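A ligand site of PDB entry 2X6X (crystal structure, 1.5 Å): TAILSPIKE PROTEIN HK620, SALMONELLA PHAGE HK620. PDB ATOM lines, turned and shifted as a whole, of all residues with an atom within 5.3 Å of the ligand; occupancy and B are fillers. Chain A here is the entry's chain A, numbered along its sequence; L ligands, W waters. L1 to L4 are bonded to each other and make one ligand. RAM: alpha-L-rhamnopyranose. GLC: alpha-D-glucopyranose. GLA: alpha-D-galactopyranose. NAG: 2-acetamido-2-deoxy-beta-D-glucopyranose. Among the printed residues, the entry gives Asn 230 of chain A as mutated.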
ATOM      1  N   GLY A 102     -17.547   5.102  -4.213  1.00  0.00           N
ATOM      2  CA  GLY A 102     -17.084   4.903  -2.839  1.00  0.00           C
ATOM      3  C   GLY A 102     -17.523   5.998  -1.866  1.00  0.00           C
ATOM      4  O   GLY A 102     -17.377   5.833  -0.642  1.00  0.00           O
ATOM      5  N   HIS A 103     -18.072   7.082  -2.398  1.00  0.00           N
ATOM      6  CA  HIS A 103     -18.549   8.203  -1.603  1.00  0.00           C
ATOM      7  C   HIS A 103     -20.069   8.307  -1.682  1.00  0.00           C
ATOM      8  O   HIS A 103     -20.634   9.340  -1.321  1.00  0.00           O
ATOM      9  CB  HIS A 103     -17.920   9.520  -2.098  1.00  0.00           C
ATOM     10  CG  HIS A 103     -16.425   9.495  -2.147  1.00  0.00           C
ATOM     11  ND1 HIS A 103     -15.636   9.830  -1.069  1.00  0.00           N
ATOM     12  CD2 HIS A 103     -15.570   9.192  -3.150  1.00  0.00           C
ATOM     13  CE1 HIS A 103     -14.359   9.736  -1.411  1.00  0.00           C
ATOM     14  NE2 HIS A 103     -14.293   9.340  -2.663  1.00  0.00           N
ATOM     15  N   GLN A 133     -24.016  11.443  -1.484  1.00  0.00           N
ATOM     16  CA  GLN A 133     -23.312  12.719  -1.532  1.00  0.00           C
ATOM     17  C   GLN A 133     -23.565  13.274  -2.902  1.00  0.00           C
ATOM     18  O   GLN A 133     -23.135  12.694  -3.897  1.00  0.00           O
ATOM     19  CB  GLN A 133     -21.815  12.549  -1.259  1.00  0.00           C
ATOM     20  CG  GLN A 133     -21.563  12.009   0.151  1.00  0.00           C
ATOM     21  CD  GLN A 133     -20.117  12.176   0.605  1.00  0.00           C
ATOM     22  OE1 GLN A 133     -19.549  13.287   0.604  1.00  0.00           O
ATOM     23  NE2 GLN A 133     -19.501  11.056   1.019  1.00  0.00           N
ATOM     24  N   PHE A 138     -13.970  14.347  -5.454  1.00  0.00           N
ATOM     25  CA  PHE A 138     -12.970  13.281  -5.486  1.00  0.00           C
ATOM     26  C   PHE A 138     -13.129  12.516  -6.798  1.00  0.00           C
ATOM     27  O   PHE A 138     -14.231  12.430  -7.330  1.00  0.00           O
ATOM     28  CB  PHE A 138     -13.195  12.293  -4.343  1.00  0.00           C
ATOM     29  CG  PHE A 138     -13.008  12.866  -2.952  1.00  0.00           C
ATOM     30  CD1 PHE A 138     -11.735  13.120  -2.456  1.00  0.00           C
ATOM     31  CD2 PHE A 138     -14.102  13.068  -2.111  1.00  0.00           C
ATOM     32  CE1 PHE A 138     -11.566  13.600  -1.155  1.00  0.00           C
ATOM     33  CE2 PHE A 138     -13.926  13.525  -0.839  1.00  0.00           C
ATOM     34  CZ  PHE A 138     -12.650  13.789  -0.357  1.00  0.00           C
ATOM     35  N   PRO A 143      -9.923   8.638  -0.866  1.00  0.00           N
ATOM     36  CA  PRO A 143      -9.496  10.033  -1.010  1.00  0.00           C
ATOM     37  C   PRO A 143      -7.977  10.228  -1.064  1.00  0.00           C
ATOM     38  O   PRO A 143      -7.507  11.162  -1.722  1.00  0.00           O
ATOM     39  CB  PRO A 143     -10.117  10.719   0.208  1.00  0.00           C
ATOM     40  CG  PRO A 143     -10.523   9.674   1.140  1.00  0.00           C
ATOM     41  CD  PRO A 143     -10.734   8.410   0.335  1.00  0.00           C
ATOM     42  N   LEU A 173     -23.752   8.172   5.780  1.00  0.00           N
ATOM     43  CA  LEU A 173     -23.321   9.553   5.606  1.00  0.00           C
ATOM     44  C   LEU A 173     -24.087  10.171   4.447  1.00  0.00           C
ATOM     45  O   LEU A 173     -24.348   9.488   3.434  1.00  0.00           O
ATOM     46  CB  LEU A 173     -21.831   9.633   5.320  1.00  0.00           C
ATOM     47  CG  LEU A 173     -20.862   9.100   6.379  1.00  0.00           C
ATOM     48  CD1 LEU A 173     -19.441   9.052   5.801  1.00  0.00           C
ATOM     49  CD2 LEU A 173     -20.901   9.913   7.663  1.00  0.00           C
ATOM     50  N   THR A 198     -25.578  14.650   6.983  1.00  0.00           N
ATOM     51  CA  THR A 198     -24.414  14.775   7.873  1.00  0.00           C
ATOM     52  C   THR A 198     -23.770  16.158   7.742  1.00  0.00           C
ATOM     53  O   THR A 198     -23.410  16.774   8.731  1.00  0.00           O
ATOM     54  CB  THR A 198     -23.346  13.722   7.550  1.00  0.00           C
ATOM     55  OG1 THR A 198     -23.931  12.403   7.466  1.00  0.00           O
ATOM     56  CG2 THR A 198     -22.260  13.717   8.610  1.00  0.00           C
ATOM     57  N   TRP A 199     -23.617  16.598   6.493  1.00  0.00           N
ATOM     58  CA  TRP A 199     -23.087  17.932   6.130  1.00  0.00           C
ATOM     59  C   TRP A 199     -23.898  18.411   4.920  1.00  0.00           C
ATOM     60  O   TRP A 199     -24.457  17.572   4.181  1.00  0.00           O
ATOM     61  CB  TRP A 199     -21.617  17.881   5.720  1.00  0.00           C
ATOM     62  CG  TRP A 199     -20.717  17.022   6.577  1.00  0.00           C
ATOM     63  CD1 TRP A 199     -20.160  17.349   7.768  1.00  0.00           C
ATOM     64  CD2 TRP A 199     -20.249  15.700   6.269  1.00  0.00           C
ATOM     65  NE1 TRP A 199     -19.377  16.322   8.228  1.00  0.00           N
ATOM     66  CE2 TRP A 199     -19.433  15.288   7.334  1.00  0.00           C
ATOM     67  CE3 TRP A 199     -20.483  14.818   5.210  1.00  0.00           C
ATOM     68  CZ2 TRP A 199     -18.821  14.039   7.362  1.00  0.00           C
ATOM     69  CZ3 TRP A 199     -19.886  13.573   5.231  1.00  0.00           C
ATOM     70  CH2 TRP A 199     -19.052  13.189   6.305  1.00  0.00           C
ATOM     71  N   THR A 202     -18.756  20.093   2.317  1.00  0.00           N
ATOM     72  CA  THR A 202     -17.437  19.884   2.887  1.00  0.00           C
ATOM     73  C   THR A 202     -16.392  20.487   1.924  1.00  0.00           C
ATOM     74  O   THR A 202     -16.537  20.395   0.685  1.00  0.00           O
ATOM     75  CB  THR A 202     -17.140  18.400   3.202  1.00  0.00           C
ATOM     76  OG1 THR A 202     -17.101  17.621   2.006  1.00  0.00           O
ATOM     77  CG2 THR A 202     -18.204  17.830   4.140  1.00  0.00           C
ATOM     78  N   GLY A 204     -12.238  20.658   1.111  1.00  0.00           N
ATOM     79  CA  GLY A 204     -10.948  20.012   1.354  1.00  0.00           C
ATOM     80  C   GLY A 204     -11.037  18.588   1.865  1.00  0.00           C
ATOM     81  O   GLY A 204     -12.119  18.053   2.106  1.00  0.00           O
ATOM     82  N   TRP A 205      -9.874  17.991   2.069  1.00  0.00           N
ATOM     83  CA  TRP A 205      -9.775  16.656   2.621  1.00  0.00           C
ATOM     84  C   TRP A 205      -8.466  16.558   3.403  1.00  0.00           C
ATOM     85  O   TRP A 205      -7.402  16.635   2.815  1.00  0.00           O
ATOM     86  CB  TRP A 205      -9.815  15.557   1.535  1.00  0.00           C
ATOM     87  CG  TRP A 205      -9.585  14.232   2.153  1.00  0.00           C
ATOM     88  CD1 TRP A 205     -10.456  13.535   2.947  1.00  0.00           C
ATOM     89  CD2 TRP A 205      -8.381  13.468   2.128  1.00  0.00           C
ATOM     90  NE1 TRP A 205      -9.880  12.383   3.380  1.00  0.00           N
ATOM     91  CE2 TRP A 205      -8.603  12.313   2.904  1.00  0.00           C
ATOM     92  CE3 TRP A 205      -7.146  13.652   1.519  1.00  0.00           C
ATOM     93  CZ2 TRP A 205      -7.624  11.341   3.069  1.00  0.00           C
ATOM     94  CZ3 TRP A 205      -6.164  12.682   1.693  1.00  0.00           C
ATOM     95  CH2 TRP A 205      -6.417  11.536   2.454  1.00  0.00           C
ATOM     96  N   ASN A 206      -8.574  16.451   4.731  1.00  0.00           N
ATOM     97  CA  ASN A 206      -7.421  16.276   5.630  1.00  0.00           C
ATOM     98  C   ASN A 206      -6.291  17.232   5.329  1.00  0.00           C
ATOM     99  O   ASN A 206      -5.132  16.869   5.245  1.00  0.00           O
ATOM    100  CB  ASN A 206      -6.968  14.810   5.628  1.00  0.00           C
ATOM    101  CG  ASN A 206      -8.005  13.898   6.255  1.00  0.00           C
ATOM    102  OD1 ASN A 206      -9.071  14.359   6.674  1.00  0.00           O
ATOM    103  ND2 ASN A 206      -7.706  12.611   6.299  1.00  0.00           N
ATOM    104  N   ASN A 230     -25.079  12.763  13.714  1.00  0.00           N
ATOM    105  CA  ASN A 230     -24.302  13.996  13.868  1.00  0.00           C
ATOM    106  C   ASN A 230     -24.469  14.854  12.636  1.00  0.00           C
ATOM    107  O   ASN A 230     -24.636  14.337  11.525  1.00  0.00           O
ATOM    108  CB  ASN A 230     -22.825  13.639  14.063  1.00  0.00           C
ATOM    109  CG  ASN A 230     -21.951  14.866  14.329  1.00  0.00           C
ATOM    110  OD1 ASN A 230     -22.330  15.775  15.049  1.00  0.00           O
ATOM    111  ND2 ASN A 230     -20.759  14.867  13.732  1.00  0.00           N
ATOM    112  N   TYR A 235     -18.168  21.895   6.721  1.00  0.00           N
ATOM    113  CA  TYR A 235     -16.958  21.337   7.330  1.00  0.00           C
ATOM    114  C   TYR A 235     -15.764  21.828   6.510  1.00  0.00           C
ATOM    115  O   TYR A 235     -15.621  21.477   5.322  1.00  0.00           O
ATOM    116  CB  TYR A 235     -17.021  19.810   7.345  1.00  0.00           C
ATOM    117  CG  TYR A 235     -16.086  19.079   8.278  1.00  0.00           C
ATOM    118  CD1 TYR A 235     -14.734  18.942   7.987  1.00  0.00           C
ATOM    119  CD2 TYR A 235     -16.563  18.467   9.439  1.00  0.00           C
ATOM    120  CE1 TYR A 235     -13.884  18.245   8.831  1.00  0.00           C
ATOM    121  CE2 TYR A 235     -15.722  17.756  10.278  1.00  0.00           C
ATOM    122  CZ  TYR A 235     -14.382  17.645   9.974  1.00  0.00           C
ATOM    123  OH  TYR A 235     -13.547  16.922  10.817  1.00  0.00           O
ATOM    124  N   ASN A 237     -12.086  21.708   5.799  1.00  0.00           N
ATOM    125  CA  ASN A 237     -10.946  20.818   6.015  1.00  0.00           C
ATOM    126  C   ASN A 237      -9.764  21.107   5.065  1.00  0.00           C
ATOM    127  O   ASN A 237      -8.970  20.240   4.736  1.00  0.00           O
ATOM    128  CB  ASN A 237     -11.378  19.348   5.932  1.00  0.00           C
ATOM    129  CG  ASN A 237     -10.529  18.440   6.794  1.00  0.00           C
ATOM    130  OD1 ASN A 237      -9.658  18.892   7.521  1.00  0.00           O
ATOM    131  ND2 ASN A 237     -10.795  17.144   6.728  1.00  0.00           N
ATOM    132  N   GLU A 263     -17.611  23.665  11.046  1.00  0.00           N
ATOM    133  CA  GLU A 263     -16.389  23.214  11.711  1.00  0.00           C
ATOM    134  C   GLU A 263     -15.194  23.778  10.949  1.00  0.00           C
ATOM    135  O   GLU A 263     -15.123  23.693   9.708  1.00  0.00           O
ATOM    136  CB  GLU A 263     -16.271  21.707  11.817  1.00  0.00           C
ATOM    137  CG  GLU A 263     -17.493  21.045  12.397  1.00  0.00           C
ATOM    138  CD  GLU A 263     -17.212  19.642  12.944  1.00  0.00           C
ATOM    139  OE1 GLU A 263     -16.077  19.357  13.403  1.00  0.00           O
ATOM    140  OE2 GLU A 263     -18.148  18.812  12.934  1.00  0.00           O
ATOM    141  N   HIS A 288      -7.591  18.119  14.586  1.00  0.00           N
ATOM    142  CA  HIS A 288      -7.579  16.660  14.680  1.00  0.00           C
ATOM    143  C   HIS A 288      -6.275  16.166  14.071  1.00  0.00           C
ATOM    144  O   HIS A 288      -6.052  16.363  12.890  1.00  0.00           O
ATOM    145  CB  HIS A 288      -8.721  16.044  13.868  1.00  0.00           C
ATOM    146  CG  HIS A 288     -10.080  16.161  14.486  1.00  0.00           C
ATOM    147  ND1 HIS A 288     -10.340  15.887  15.813  1.00  0.00           N
ATOM    148  CD2 HIS A 288     -11.276  16.454  13.925  1.00  0.00           C
ATOM    149  CE1 HIS A 288     -11.629  16.036  16.040  1.00  0.00           C
ATOM    150  NE2 HIS A 288     -12.220  16.386  14.913  1.00  0.00           N
ATOM    151  N   ALA A 290      -5.673  13.222  13.155  1.00  0.00           N
ATOM    152  CA  ALA A 290      -6.044  12.360  12.035  1.00  0.00           C
ATOM    153  C   ALA A 290      -6.250  13.118  10.710  1.00  0.00           C
ATOM    154  O   ALA A 290      -6.326  12.488   9.641  1.00  0.00           O
ATOM    155  CB  ALA A 290      -7.298  11.538  12.373  1.00  0.00           C
ATOM    156  N   GLU A 291      -6.346  14.454  10.776  1.00  0.00           N
ATOM    157  CA  GLU A 291      -6.544  15.299   9.599  1.00  0.00           C
ATOM    158  C   GLU A 291      -5.323  16.166   9.206  1.00  0.00           C
ATOM    159  O   GLU A 291      -5.440  17.066   8.388  1.00  0.00           O
ATOM    160  CB  GLU A 291      -7.788  16.172   9.813  1.00  0.00           C
ATOM    161  CG  GLU A 291      -9.059  15.380  10.031  1.00  0.00           C
ATOM    162  CD  GLU A 291     -10.247  16.279  10.297  1.00  0.00           C
ATOM    163  OE1 GLU A 291     -10.048  17.403  10.808  1.00  0.00           O
ATOM    164  OE2 GLU A 291     -11.373  15.860  10.022  1.00  0.00           O
ATOM    165  N   ASN A 362     -12.785  12.923  20.917  1.00  0.00           N
ATOM    166  CA  ASN A 362     -13.936  12.071  20.569  1.00  0.00           C
ATOM    167  C   ASN A 362     -14.101  10.860  21.490  1.00  0.00           C
ATOM    168  O   ASN A 362     -15.221  10.407  21.723  1.00  0.00           O
ATOM    169  CB  ASN A 362     -13.872  11.602  19.100  1.00  0.00           C
ATOM    170  CG  ASN A 362     -14.102  12.747  18.097  1.00  0.00           C
ATOM    171  OD1 ASN A 362     -14.553  13.829  18.477  1.00  0.00           O
ATOM    172  ND2 ASN A 362     -13.795  12.491  16.828  1.00  0.00           N
HETATM  173  C1  RAM L   1     -15.090   9.067   4.924  1.00  0.00           C
HETATM  174  C2  RAM L   1     -16.017   8.207   4.063  1.00  0.00           C
HETATM  175  C3  RAM L   1     -16.742   9.031   2.993  1.00  0.00           C
HETATM  176  C4  RAM L   1     -15.754   9.933   2.255  1.00  0.00           C
HETATM  177  C5  RAM L   1     -14.937  10.777   3.258  1.00  0.00           C
HETATM  178  C6  RAM L   1     -13.853  11.601   2.574  1.00  0.00           C
HETATM  179  O2  RAM L   1     -15.218   7.240   3.457  1.00  0.00           O
HETATM  180  O3  RAM L   1     -17.408   8.193   2.050  1.00  0.00           O
HETATM  181  O4  RAM L   1     -16.499  10.732   1.356  1.00  0.00           O
HETATM  182  O5  RAM L   1     -14.252   9.916   4.157  1.00  0.00           O
HETATM  183  C1  GLC L   2     -17.636  10.397   9.538  1.00  0.00           C
HETATM  184  C2  GLC L   2     -17.554   8.909   9.864  1.00  0.00           C
HETATM  185  C3  GLC L   2     -16.115   8.411   9.750  1.00  0.00           C
HETATM  186  C4  GLC L   2     -15.575   8.748   8.369  1.00  0.00           C
HETATM  187  C5  GLC L   2     -15.725  10.255   8.112  1.00  0.00           C
HETATM  188  C6  GLC L   2     -15.346  10.706   6.708  1.00  0.00           C
HETATM  189  O2  GLC L   2     -18.017   8.770  11.187  1.00  0.00           O
HETATM  190  O3  GLC L   2     -16.037   7.014   9.982  1.00  0.00           O
HETATM  191  O4  GLC L   2     -14.229   8.375   8.307  1.00  0.00           O
HETATM  192  O5  GLC L   2     -17.079  10.617   8.265  1.00  0.00           O
HETATM  193  O6  GLC L   2     -15.867   9.855   5.790  1.00  0.00           O
HETATM  194  C1  GLA L   3     -16.202  13.282  13.075  1.00  0.00           C
HETATM  195  C2  GLA L   3     -15.130  13.178  12.004  1.00  0.00           C
HETATM  196  C3  GLA L   3     -15.845  13.286  10.650  1.00  0.00           C
HETATM  197  C4  GLA L   3     -17.167  12.483  10.598  1.00  0.00           C
HETATM  198  C5  GLA L   3     -18.136  12.914  11.721  1.00  0.00           C
HETATM  199  C6  GLA L   3     -19.390  12.056  11.876  1.00  0.00           C
HETATM  200  O1  GLA L   3     -16.454  14.669  12.961  1.00  0.00           O
HETATM  201  O2  GLA L   3     -14.169  14.185  12.158  1.00  0.00           O
HETATM  202  O3  GLA L   3     -14.922  12.910   9.655  1.00  0.00           O
HETATM  203  O4  GLA L   3     -16.959  11.160  10.516  1.00  0.00           O
HETATM  204  O5  GLA L   3     -17.566  12.954  13.030  1.00  0.00           O
HETATM  205  O6  GLA L   3     -20.470  12.651  11.230  1.00  0.00           O
HETATM  206  C1  NAG L   4     -14.366  13.857   8.884  1.00  0.00           C
HETATM  207  C2  NAG L   4     -13.074  13.297   8.283  1.00  0.00           C
HETATM  208  C3  NAG L   4     -12.461  14.138   7.157  1.00  0.00           C
HETATM  209  C4  NAG L   4     -13.525  14.700   6.226  1.00  0.00           C
HETATM  210  C5  NAG L   4     -14.709  15.225   7.006  1.00  0.00           C
HETATM  211  C6  NAG L   4     -15.797  15.805   6.111  1.00  0.00           C
HETATM  212  C7  NAG L   4     -11.698  11.938   9.769  1.00  0.00           C
HETATM  213  C8  NAG L   4     -10.657  11.920  10.845  1.00  0.00           C
HETATM  214  N2  NAG L   4     -12.079  13.132   9.333  1.00  0.00           N
HETATM  215  O3  NAG L   4     -11.516  13.361   6.431  1.00  0.00           O
HETATM  216  O4  NAG L   4     -12.933  15.735   5.466  1.00  0.00           O
HETATM  217  O5  NAG L   4     -15.267  14.225   7.855  1.00  0.00           O
HETATM  218  O6  NAG L   4     -16.340  14.801   5.288  1.00  0.00           O
HETATM  219  O7  NAG L   4     -12.166  10.884   9.332  1.00  0.00           O
HETATM  220  O   HOH W   1     -20.100   6.950  10.583  1.00  0.00           O
HETATM  221  O   HOH W   2     -15.348  16.875  14.297  1.00  0.00           O
HETATM  222  O   HOH W   3     -16.040  15.249   2.594  1.00  0.00           O
HETATM  223  O   HOH W   4     -22.492  11.022  11.247  1.00  0.00           O
HETATM  224  O   HOH W   5     -15.068   6.447   0.907  1.00  0.00           O
HETATM  225  O   HOH W   6     -21.554  15.696  11.100  1.00  0.00           O
HETATM  226  O   HOH W   7     -10.270   9.684  13.331  1.00  0.00           O
HETATM  227  O   HOH W   8     -13.202  15.566   2.817  1.00  0.00           O
HETATM  228  O   HOH W   9     -11.722  10.707   5.236  1.00  0.00           O
HETATM  229  O   HOH W  10     -20.334   7.783   1.906  1.00  0.00           O
HETATM  230  O   HOH W  11     -16.881  13.358   0.989  1.00  0.00           O
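O3 of NAG L4 is in hydrogen-bond range of OD1 of Asn 206 (2.7 Å). ND1 of His 103 sits at hydrogen-bond distance from O4 of RAM L1, 2.7 Å away. O4 of NAG L4 lies within hydrogen-bond range of ND2 of Asn 237. The side-chain carboxylate (OE2) of Glu 291 is in hydrogen-bond range of a nitrogen (N2) of NAG L4 (2.9 Å). NE2 of Gln 133 lies within hydrogen-bond range of O4 of RAM L1 (3.0 Å). The side-chain hydroxyl (OH) of Tyr 235 sits at hydrogen-bond distance from an oxygen (O2) of GLA L3, 3.1 Å away. An oxygen (O6) of GLA L3 lies within hydrogen-bond range of the side-chain amide nitrogen (ND2) of Asn 230.
Water W8 bridges O4 of NAG L4 (2.7 Å) and O of Gly 204 (2.8 Å). Water W5 bridges an oxygen (O2) of RAM L1 and the backbone carbonyl oxygen (O) of Gly 102. Water W11 bridges O4 of RAM L1 and OE1 of Gln 133. Water W3 bridges OG1 of Thr 202 (2.7 Å) and O6 of NAG L4 (2.7 Å). Water W9 bridges O5 of RAM L1 and NE1 of Trp 205. Water W10 lies within hydrogen-bond range of an oxygen (O3) of RAM L1 (3.0 Å) and the side-chain amide nitrogen (NE2) of Gln 133 (3.5 Å).
O of Gly 102 touches O3 of RAM L1 (3.6 Å). CZ of Phe 138 touches C6 of RAM L1, at 3.9 Å. CD1 of Leu 173 touches O6 of GLC L2 (3.7 Å). Thr 198 touches the ligand. CH2 of Trp 199 touches O6 of NAG L4, at 3.3 Å. CG2 of Thr 202 touches C6 of NAG L4, at 3.7 Å. NE1 of Trp 205 touches O3 of NAG L4, 3.6 Å away. CB of Ala 290 touches C8 of NAG L4, 3.7 Å away.
The backbone NH (N) of Asn 206 sits close to the side-chain amide nitrogen (ND2) of Asn 237 (3.1 Å). The backbone carbonyl oxygen of His 103 lies within hydrogen-bond range of the side-chain amide nitrogen of Gln 133, at 3.1 Å. OE2 of Glu 291 sits at hydrogen-bond distance from OH of Tyr 235 (2.5 Å).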
